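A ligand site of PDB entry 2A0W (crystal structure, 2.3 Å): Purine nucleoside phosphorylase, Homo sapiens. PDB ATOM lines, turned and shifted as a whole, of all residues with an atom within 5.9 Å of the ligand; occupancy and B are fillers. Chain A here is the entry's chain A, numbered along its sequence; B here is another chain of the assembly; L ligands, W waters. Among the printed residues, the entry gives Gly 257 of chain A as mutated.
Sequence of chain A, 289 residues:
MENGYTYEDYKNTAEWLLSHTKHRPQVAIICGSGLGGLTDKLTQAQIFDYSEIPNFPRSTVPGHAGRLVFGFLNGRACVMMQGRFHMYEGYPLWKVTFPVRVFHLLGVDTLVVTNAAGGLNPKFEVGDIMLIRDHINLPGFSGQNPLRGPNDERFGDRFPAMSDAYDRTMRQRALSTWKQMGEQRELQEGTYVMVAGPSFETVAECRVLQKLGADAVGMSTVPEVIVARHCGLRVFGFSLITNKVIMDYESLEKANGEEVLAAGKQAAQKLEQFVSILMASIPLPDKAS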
ATOM      1  N   SER A  33      -6.601 -18.077  21.458  1.00  0.00           N
ATOM      2  CA  SER A  33      -6.328 -17.212  22.608  1.00  0.00           C
ATOM      3  C   SER A  33      -6.383 -15.722  22.270  1.00  0.00           C
ATOM      4  O   SER A  33      -5.730 -15.261  21.335  1.00  0.00           O
ATOM      5  CB  SER A  33      -4.952 -17.547  23.195  1.00  0.00           C
ATOM      6  OG  SER A  33      -4.623 -16.650  24.234  1.00  0.00           O
ATOM      7  N   HIS A  86      -7.268 -27.842  25.238  1.00  0.00           N
ATOM      8  CA  HIS A  86      -5.881 -28.142  24.896  1.00  0.00           C
ATOM      9  C   HIS A  86      -5.391 -29.430  25.548  1.00  0.00           C
ATOM     10  O   HIS A  86      -5.758 -29.765  26.672  1.00  0.00           O
ATOM     11  CB  HIS A  86      -4.934 -27.026  25.361  1.00  0.00           C
ATOM     12  CG  HIS A  86      -5.325 -25.654  24.898  1.00  0.00           C
ATOM     13  ND1 HIS A  86      -6.314 -24.922  25.519  1.00  0.00           N
ATOM     14  CD2 HIS A  86      -4.821 -24.870  23.919  1.00  0.00           C
ATOM     15  CE1 HIS A  86      -6.405 -23.740  24.931  1.00  0.00           C
ATOM     16  NE2 HIS A  86      -5.505 -23.680  23.965  1.00  0.00           N
ATOM     17  N   TYR A  88      -2.531 -29.991  26.776  1.00  0.00           N
ATOM     18  CA  TYR A  88      -1.782 -29.693  27.997  1.00  0.00           C
ATOM     19  C   TYR A  88      -2.623 -29.567  29.268  1.00  0.00           C
ATOM     20  O   TYR A  88      -2.085 -29.691  30.364  1.00  0.00           O
ATOM     21  CB  TYR A  88      -0.906 -28.431  27.819  1.00  0.00           C
ATOM     22  CG  TYR A  88      -1.635 -27.122  27.578  1.00  0.00           C
ATOM     23  CD1 TYR A  88      -2.451 -26.538  28.553  1.00  0.00           C
ATOM     24  CD2 TYR A  88      -1.518 -26.463  26.354  1.00  0.00           C
ATOM     25  CE1 TYR A  88      -3.130 -25.335  28.313  1.00  0.00           C
ATOM     26  CE2 TYR A  88      -2.189 -25.261  26.091  1.00  0.00           C
ATOM     27  CZ  TYR A  88      -2.996 -24.708  27.070  1.00  0.00           C
ATOM     28  OH  TYR A  88      -3.659 -23.534  26.797  1.00  0.00           O
ATOM     29  N   ALA A 116      -3.152 -18.294  18.456  1.00  0.00           N
ATOM     30  CA  ALA A 116      -2.045 -17.378  18.677  1.00  0.00           C
ATOM     31  C   ALA A 116      -0.851 -18.314  18.534  1.00  0.00           C
ATOM     32  O   ALA A 116      -0.963 -19.498  18.830  1.00  0.00           O
ATOM     33  CB  ALA A 116      -2.111 -16.808  20.092  1.00  0.00           C
ATOM     34  N   ALA A 117       0.290 -17.801  18.076  1.00  0.00           N
ATOM     35  CA  ALA A 117       1.461 -18.651  17.917  1.00  0.00           C
ATOM     36  C   ALA A 117       2.767 -17.877  18.017  1.00  0.00           C
ATOM     37  O   ALA A 117       2.799 -16.666  17.859  1.00  0.00           O
ATOM     38  CB  ALA A 117       1.401 -19.365  16.563  1.00  0.00           C
ATOM     39  N   GLY A 118       3.838 -18.603  18.305  1.00  0.00           N
ATOM     40  CA  GLY A 118       5.143 -17.990  18.396  1.00  0.00           C
ATOM     41  C   GLY A 118       5.710 -18.054  17.006  1.00  0.00           C
ATOM     42  O   GLY A 118       5.521 -19.049  16.302  1.00  0.00           O
ATOM     43  N   GLY A 119       6.380 -16.987  16.584  1.00  0.00           N
ATOM     44  CA  GLY A 119       6.950 -16.961  15.254  1.00  0.00           C
ATOM     45  C   GLY A 119       8.326 -17.582  15.201  1.00  0.00           C
ATOM     46  O   GLY A 119       9.212 -17.209  15.965  1.00  0.00           O
ATOM     47  N   VAL A 195       3.136 -28.471  19.286  1.00  0.00           N
ATOM     48  CA  VAL A 195       3.914 -29.107  20.352  1.00  0.00           C
ATOM     49  C   VAL A 195       2.928 -29.103  21.506  1.00  0.00           C
ATOM     50  O   VAL A 195       2.073 -28.215  21.592  1.00  0.00           O
ATOM     51  CB  VAL A 195       5.192 -28.317  20.764  1.00  0.00           C
ATOM     52  CG1 VAL A 195       6.208 -28.328  19.622  1.00  0.00           C
ATOM     53  CG2 VAL A 195       4.826 -26.912  21.184  1.00  0.00           C
ATOM     54  N   PHE A 200       7.018 -23.139  27.647  1.00  0.00           N
ATOM     55  CA  PHE A 200       7.541 -22.595  26.393  1.00  0.00           C
ATOM     56  C   PHE A 200       8.863 -23.213  25.971  1.00  0.00           C
ATOM     57  O   PHE A 200       9.618 -23.742  26.798  1.00  0.00           O
ATOM     58  CB  PHE A 200       7.687 -21.066  26.493  1.00  0.00           C
ATOM     59  CG  PHE A 200       6.380 -20.330  26.455  1.00  0.00           C
ATOM     60  CD1 PHE A 200       5.536 -20.433  25.354  1.00  0.00           C
ATOM     61  CD2 PHE A 200       5.982 -19.543  27.536  1.00  0.00           C
ATOM     62  CE1 PHE A 200       4.306 -19.764  25.321  1.00  0.00           C
ATOM     63  CE2 PHE A 200       4.753 -18.856  27.516  1.00  0.00           C
ATOM     64  CZ  PHE A 200       3.914 -18.973  26.395  1.00  0.00           C
ATOM     65  N   GLU A 201       9.151 -23.129  24.684  1.00  0.00           N
ATOM     66  CA  GLU A 201      10.360 -23.705  24.108  1.00  0.00           C
ATOM     67  C   GLU A 201      11.692 -23.098  24.554  1.00  0.00           C
ATOM     68  O   GLU A 201      11.779 -21.919  24.890  1.00  0.00           O
ATOM     69  CB  GLU A 201      10.309 -23.646  22.579  1.00  0.00           C
ATOM     70  CG  GLU A 201       9.087 -24.293  21.921  1.00  0.00           C
ATOM     71  CD  GLU A 201       7.785 -23.555  22.204  1.00  0.00           C
ATOM     72  OE1 GLU A 201       7.800 -22.340  22.473  1.00  0.00           O
ATOM     73  OE2 GLU A 201       6.723 -24.205  22.137  1.00  0.00           O
ATOM     74  N   VAL A 217       4.666 -21.739  15.908  1.00  0.00           N
ATOM     75  CA  VAL A 217       4.477 -22.821  16.867  1.00  0.00           C
ATOM     76  C   VAL A 217       3.348 -22.548  17.854  1.00  0.00           C
ATOM     77  O   VAL A 217       3.217 -21.440  18.376  1.00  0.00           O
ATOM     78  CB  VAL A 217       5.772 -23.088  17.665  1.00  0.00           C
ATOM     79  CG1 VAL A 217       6.184 -21.838  18.417  1.00  0.00           C
ATOM     80  CG2 VAL A 217       5.586 -24.260  18.602  1.00  0.00           C
ATOM     81  N   GLY A 218       2.523 -23.571  18.080  1.00  0.00           N
ATOM     82  CA  GLY A 218       1.411 -23.461  19.012  1.00  0.00           C
ATOM     83  C   GLY A 218       1.150 -24.795  19.689  1.00  0.00           C
ATOM     84  O   GLY A 218       1.853 -25.790  19.438  1.00  0.00           O
ATOM     85  N   MET A 219       0.127 -24.834  20.524  1.00  0.00           N
ATOM     86  CA  MET A 219      -0.195 -26.034  21.270  1.00  0.00           C
ATOM     87  C   MET A 219      -1.613 -26.546  21.015  1.00  0.00           C
ATOM     88  O   MET A 219      -2.212 -27.194  21.871  1.00  0.00           O
ATOM     89  CB  MET A 219      -0.013 -25.752  22.773  1.00  0.00           C
ATOM     90  CG  MET A 219       1.314 -25.109  23.112  1.00  0.00           C
ATOM     91  SD  MET A 219       1.420 -24.638  24.831  1.00  0.00           S
ATOM     92  CE  MET A 219       3.087 -24.026  24.872  1.00  0.00           C
ATOM     93  N   THR A 242       1.998 -13.706  18.139  1.00  0.00           N
ATOM     94  CA  THR A 242       1.991 -12.871  19.341  1.00  0.00           C
ATOM     95  C   THR A 242       3.399 -12.626  19.888  1.00  0.00           C
ATOM     96  O   THR A 242       3.581 -11.810  20.787  1.00  0.00           O
ATOM     97  CB  THR A 242       1.157 -13.513  20.461  1.00  0.00           C
ATOM     98  OG1 THR A 242       1.708 -14.801  20.782  1.00  0.00           O
ATOM     99  CG2 THR A 242      -0.299 -13.682  20.038  1.00  0.00           C
ATOM    100  N   ASN A 243       4.375 -13.327  19.353  1.00  0.00           N
ATOM    101  CA  ASN A 243       5.739 -13.182  19.838  1.00  0.00           C
ATOM    102  C   ASN A 243       6.731 -13.894  18.934  1.00  0.00           C
ATOM    103  O   ASN A 243       6.361 -14.810  18.203  1.00  0.00           O
ATOM    104  CB  ASN A 243       5.848 -13.766  21.251  1.00  0.00           C
ATOM    105  CG  ASN A 243       5.381 -15.224  21.320  1.00  0.00           C
ATOM    106  OD1 ASN A 243       4.218 -15.528  21.020  1.00  0.00           O
ATOM    107  ND2 ASN A 243       6.281 -16.122  21.684  1.00  0.00           N
ATOM    108  N   VAL A 245       9.785 -16.247  18.971  1.00  0.00           N
ATOM    109  CA  VAL A 245      10.503 -17.167  19.826  1.00  0.00           C
ATOM    110  C   VAL A 245      11.998 -16.867  19.836  1.00  0.00           C
ATOM    111  O   VAL A 245      12.580 -16.586  18.791  1.00  0.00           O
ATOM    112  CB  VAL A 245      10.272 -18.633  19.377  1.00  0.00           C
ATOM    113  CG1 VAL A 245       8.779 -18.938  19.350  1.00  0.00           C
ATOM    114  CG2 VAL A 245      10.860 -18.860  17.999  1.00  0.00           C
ATOM    115  N   ALA A 255       9.428 -15.658  26.969  1.00  0.00           N
ATOM    116  CA  ALA A 255       8.068 -15.695  26.430  1.00  0.00           C
ATOM    117  C   ALA A 255       7.122 -15.877  27.618  1.00  0.00           C
ATOM    118  O   ALA A 255       7.402 -16.649  28.537  1.00  0.00           O
ATOM    119  CB  ALA A 255       7.932 -16.865  25.450  1.00  0.00           C
ATOM    120  N   ASN A 256       6.003 -15.161  27.603  1.00  0.00           N
ATOM    121  CA  ASN A 256       5.045 -15.249  28.696  1.00  0.00           C
ATOM    122  C   ASN A 256       3.592 -15.172  28.228  1.00  0.00           C
ATOM    123  O   ASN A 256       3.265 -14.443  27.296  1.00  0.00           O
ATOM    124  CB  ASN A 256       5.326 -14.137  29.711  1.00  0.00           C
ATOM    125  CG  ASN A 256       5.459 -12.768  29.051  1.00  0.00           C
ATOM    126  OD1 ASN A 256       4.491 -12.216  28.522  1.00  0.00           O
ATOM    127  ND2 ASN A 256       6.667 -12.217  29.080  1.00  0.00           N
ATOM    128  N   GLY A 257       2.722 -15.948  28.880  1.00  0.00           N
ATOM    129  CA  GLY A 257       1.314 -15.954  28.531  1.00  0.00           C
ATOM    130  C   GLY A 257       0.672 -14.582  28.659  1.00  0.00           C
ATOM    131  O   GLY A 257      -0.446 -14.361  28.204  1.00  0.00           O
ATOM    132  N   GLU A 258       1.405 -13.658  29.283  1.00  0.00           N
ATOM    133  CA  GLU A 258       0.917 -12.300  29.483  1.00  0.00           C
ATOM    134  C   GLU A 258       0.929 -11.527  28.159  1.00  0.00           C
ATOM    135  O   GLU A 258      -0.089 -10.975  27.751  1.00  0.00           O
ATOM    136  CB  GLU A 258       1.796 -11.567  30.501  1.00  0.00           C
ATOM    137  CG  GLU A 258       1.997 -12.341  31.810  1.00  0.00           C
ATOM    138  CD  GLU A 258       0.690 -12.636  32.518  1.00  0.00           C
ATOM    139  OE1 GLU A 258       0.019 -11.691  32.974  1.00  0.00           O
ATOM    140  OE2 GLU A 258       0.329 -13.836  32.624  1.00  0.00           O
ATOM    141  N   VAL A 260       1.225 -12.723  25.120  1.00  0.00           N
ATOM    142  CA  VAL A 260       0.397 -13.405  24.124  1.00  0.00           C
ATOM    143  C   VAL A 260      -1.029 -12.862  24.138  1.00  0.00           C
ATOM    144  O   VAL A 260      -1.646 -12.698  23.081  1.00  0.00           O
ATOM    145  CB  VAL A 260       0.365 -14.934  24.378  1.00  0.00           C
ATOM    146  CG1 VAL A 260      -0.506 -15.610  23.326  1.00  0.00           C
ATOM    147  CG2 VAL A 260       1.782 -15.495  24.344  1.00  0.00           C
ATOM    148  N   LEU A 261      -1.548 -12.583  25.322  1.00  0.00           N
ATOM    149  CA  LEU A 261      -2.905 -12.048  25.450  1.00  0.00           C
ATOM    150  C   LEU A 261      -2.897 -10.553  25.148  1.00  0.00           C
ATOM    151  O   LEU A 261      -3.931  -9.978  24.786  1.00  0.00           O
ATOM    152  CB  LEU A 261      -3.462 -12.303  26.853  1.00  0.00           C
ATOM    153  CG  LEU A 261      -3.913 -13.729  27.163  1.00  0.00           C
ATOM    154  CD1 LEU A 261      -4.297 -13.847  28.628  1.00  0.00           C
ATOM    155  CD2 LEU A 261      -5.091 -14.107  26.266  1.00  0.00           C
ATOM    156  N   PHE B 159       2.041 -21.301  32.001  1.00  0.00           N
ATOM    157  CA  PHE B 159       3.003 -21.366  30.910  1.00  0.00           C
ATOM    158  C   PHE B 159       4.425 -20.885  31.259  1.00  0.00           C
ATOM    159  O   PHE B 159       4.867 -19.858  30.765  1.00  0.00           O
ATOM    160  CB  PHE B 159       2.481 -20.540  29.726  1.00  0.00           C
ATOM    161  CG  PHE B 159       1.068 -20.851  29.336  1.00  0.00           C
ATOM    162  CD1 PHE B 159       0.740 -22.056  28.716  1.00  0.00           C
ATOM    163  CD2 PHE B 159       0.047 -19.925  29.590  1.00  0.00           C
ATOM    164  CE1 PHE B 159      -0.586 -22.341  28.354  1.00  0.00           C
ATOM    165  CE2 PHE B 159      -1.281 -20.201  29.231  1.00  0.00           C
ATOM    166  CZ  PHE B 159      -1.600 -21.416  28.615  1.00  0.00           C
HETATM  167  O1  LIG L   1      -0.140 -17.588  26.153  1.00  0.00           O
HETATM  168  C1  LIG L   1      -0.225 -18.987  25.915  1.00  0.00           C
HETATM  169  C2  LIG L   1      -1.142 -19.703  24.978  1.00  0.00           C
HETATM  170  C3  LIG L   1      -0.894 -19.227  23.599  1.00  0.00           C
HETATM  171  C4  LIG L   1      -0.972 -21.175  24.975  1.00  0.00           C
HETATM  172  O2  LIG L   1      -2.170 -21.955  24.952  1.00  0.00           O
HETATM  173  C5  LIG L   1      -0.034 -21.221  23.839  1.00  0.00           C
HETATM  174  N1  LIG L   1      -0.608 -20.396  22.806  1.00  0.00           N
HETATM  175  C6  LIG L   1       0.246 -20.073  21.676  1.00  0.00           C
HETATM  176  C7  LIG L   1       1.609 -19.492  21.650  1.00  0.00           C
HETATM  177  C8  LIG L   1       2.007 -18.173  21.516  1.00  0.00           C
HETATM  178  N2  LIG L   1       3.304 -17.986  21.533  1.00  0.00           N
HETATM  179  C9  LIG L   1       3.838 -19.256  21.689  1.00  0.00           C
HETATM  180  C10 LIG L   1       5.233 -19.703  21.783  1.00  0.00           C
HETATM  181  O3  LIG L   1       6.235 -18.996  21.730  1.00  0.00           O
HETATM  182  N3  LIG L   1       5.386 -21.114  21.942  1.00  0.00           N
HETATM  183  C11 LIG L   1       4.311 -22.045  22.013  1.00  0.00           C
HETATM  184  N4  LIG L   1       3.002 -21.622  21.931  1.00  0.00           N
HETATM  185  C12 LIG L   1       2.814 -20.218  21.763  1.00  0.00           C
HETATM  186  O   HOH W   1      -2.077 -23.227  22.125  1.00  0.00           O
HETATM  187  O   HOH W   2       8.613 -19.683  22.865  1.00  0.00           O
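A nitrogen (N2) of the ligand lies within hydrogen-bond range of the side-chain amide oxygen (OD1) of Asn 243 (2.7 Å). A nitrogen (N3) of the ligand sits at hydrogen-bond distance from the side-chain carboxylate (OE1) of Glu 201. The side-chain hydroxyl (OH) of Tyr 88 sits at hydrogen-bond distance from an oxygen (O2) of the ligand, 2.8 Å away. The backbone NH of Gly 118 sits close to a nitrogen (N2) of the ligand.
The backbone carbonyl oxygen of Asn 243 sits at hydrogen-bond distance from the backbone NH of Gly 119. O of Gly 119 lies close to N of Val 245 (3.2 Å). O of Gly 118 is in hydrogen-bond range of N of Val 217, at 2.8 Å. OG1 of Thr 242 lies within hydrogen-bond range of OD1 of Asn 243, 2.6 Å away. OH of Tyr 88 sits at hydrogen-bond distance from ND1 of His 86 (3.3 Å). The backbone carbonyl oxygen of Gly 218 is in hydrogen-bond range of the backbone NH of Val 195 (3.0 Å). N of Thr 242 is in hydrogen-bond range of O of Ala 117.
NE2 of His 86 touches O2 of the ligand, 3.9 Å away. Ala 116 touches the ligand. C of Ala 117 touches N2 of the ligand (3.6 Å). CD1 of Phe 200 touches N3 of the ligand, at 3.5 Å. O of Val 217 touches N4 of the ligand (3.6 Å). Gly 218 touches the ligand. Met 219 touches the ligand (CE to C11, 3.7 Å). Thr 242 touches the ligand (OG1 to C8, 3.5 Å). Val 245 touches the ligand (CG1 to O3, 3.5 Å). CA of Gly 257 touches O1 of the ligand, at 3.2 Å. Val 260 touches the ligand. CE1 of Phe 159 of chain B touches C4 of the ligand, 3.6 Å away. Hydrophobic or aromatic side chains that line the ligand: Tyr 88, Phe 200, Val 217, Met 219, Val 245, Val 260 and Phe 159 of chain B.
Water W2 lies within hydrogen-bond range of an oxygen (O3) of the ligand and the side-chain carboxylate of Glu 201. Water W1 lies within hydrogen-bond range of an oxygen (O2) of the ligand (3.1 Å) and the backbone NH (N) of Met 219 (3.2 Å).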
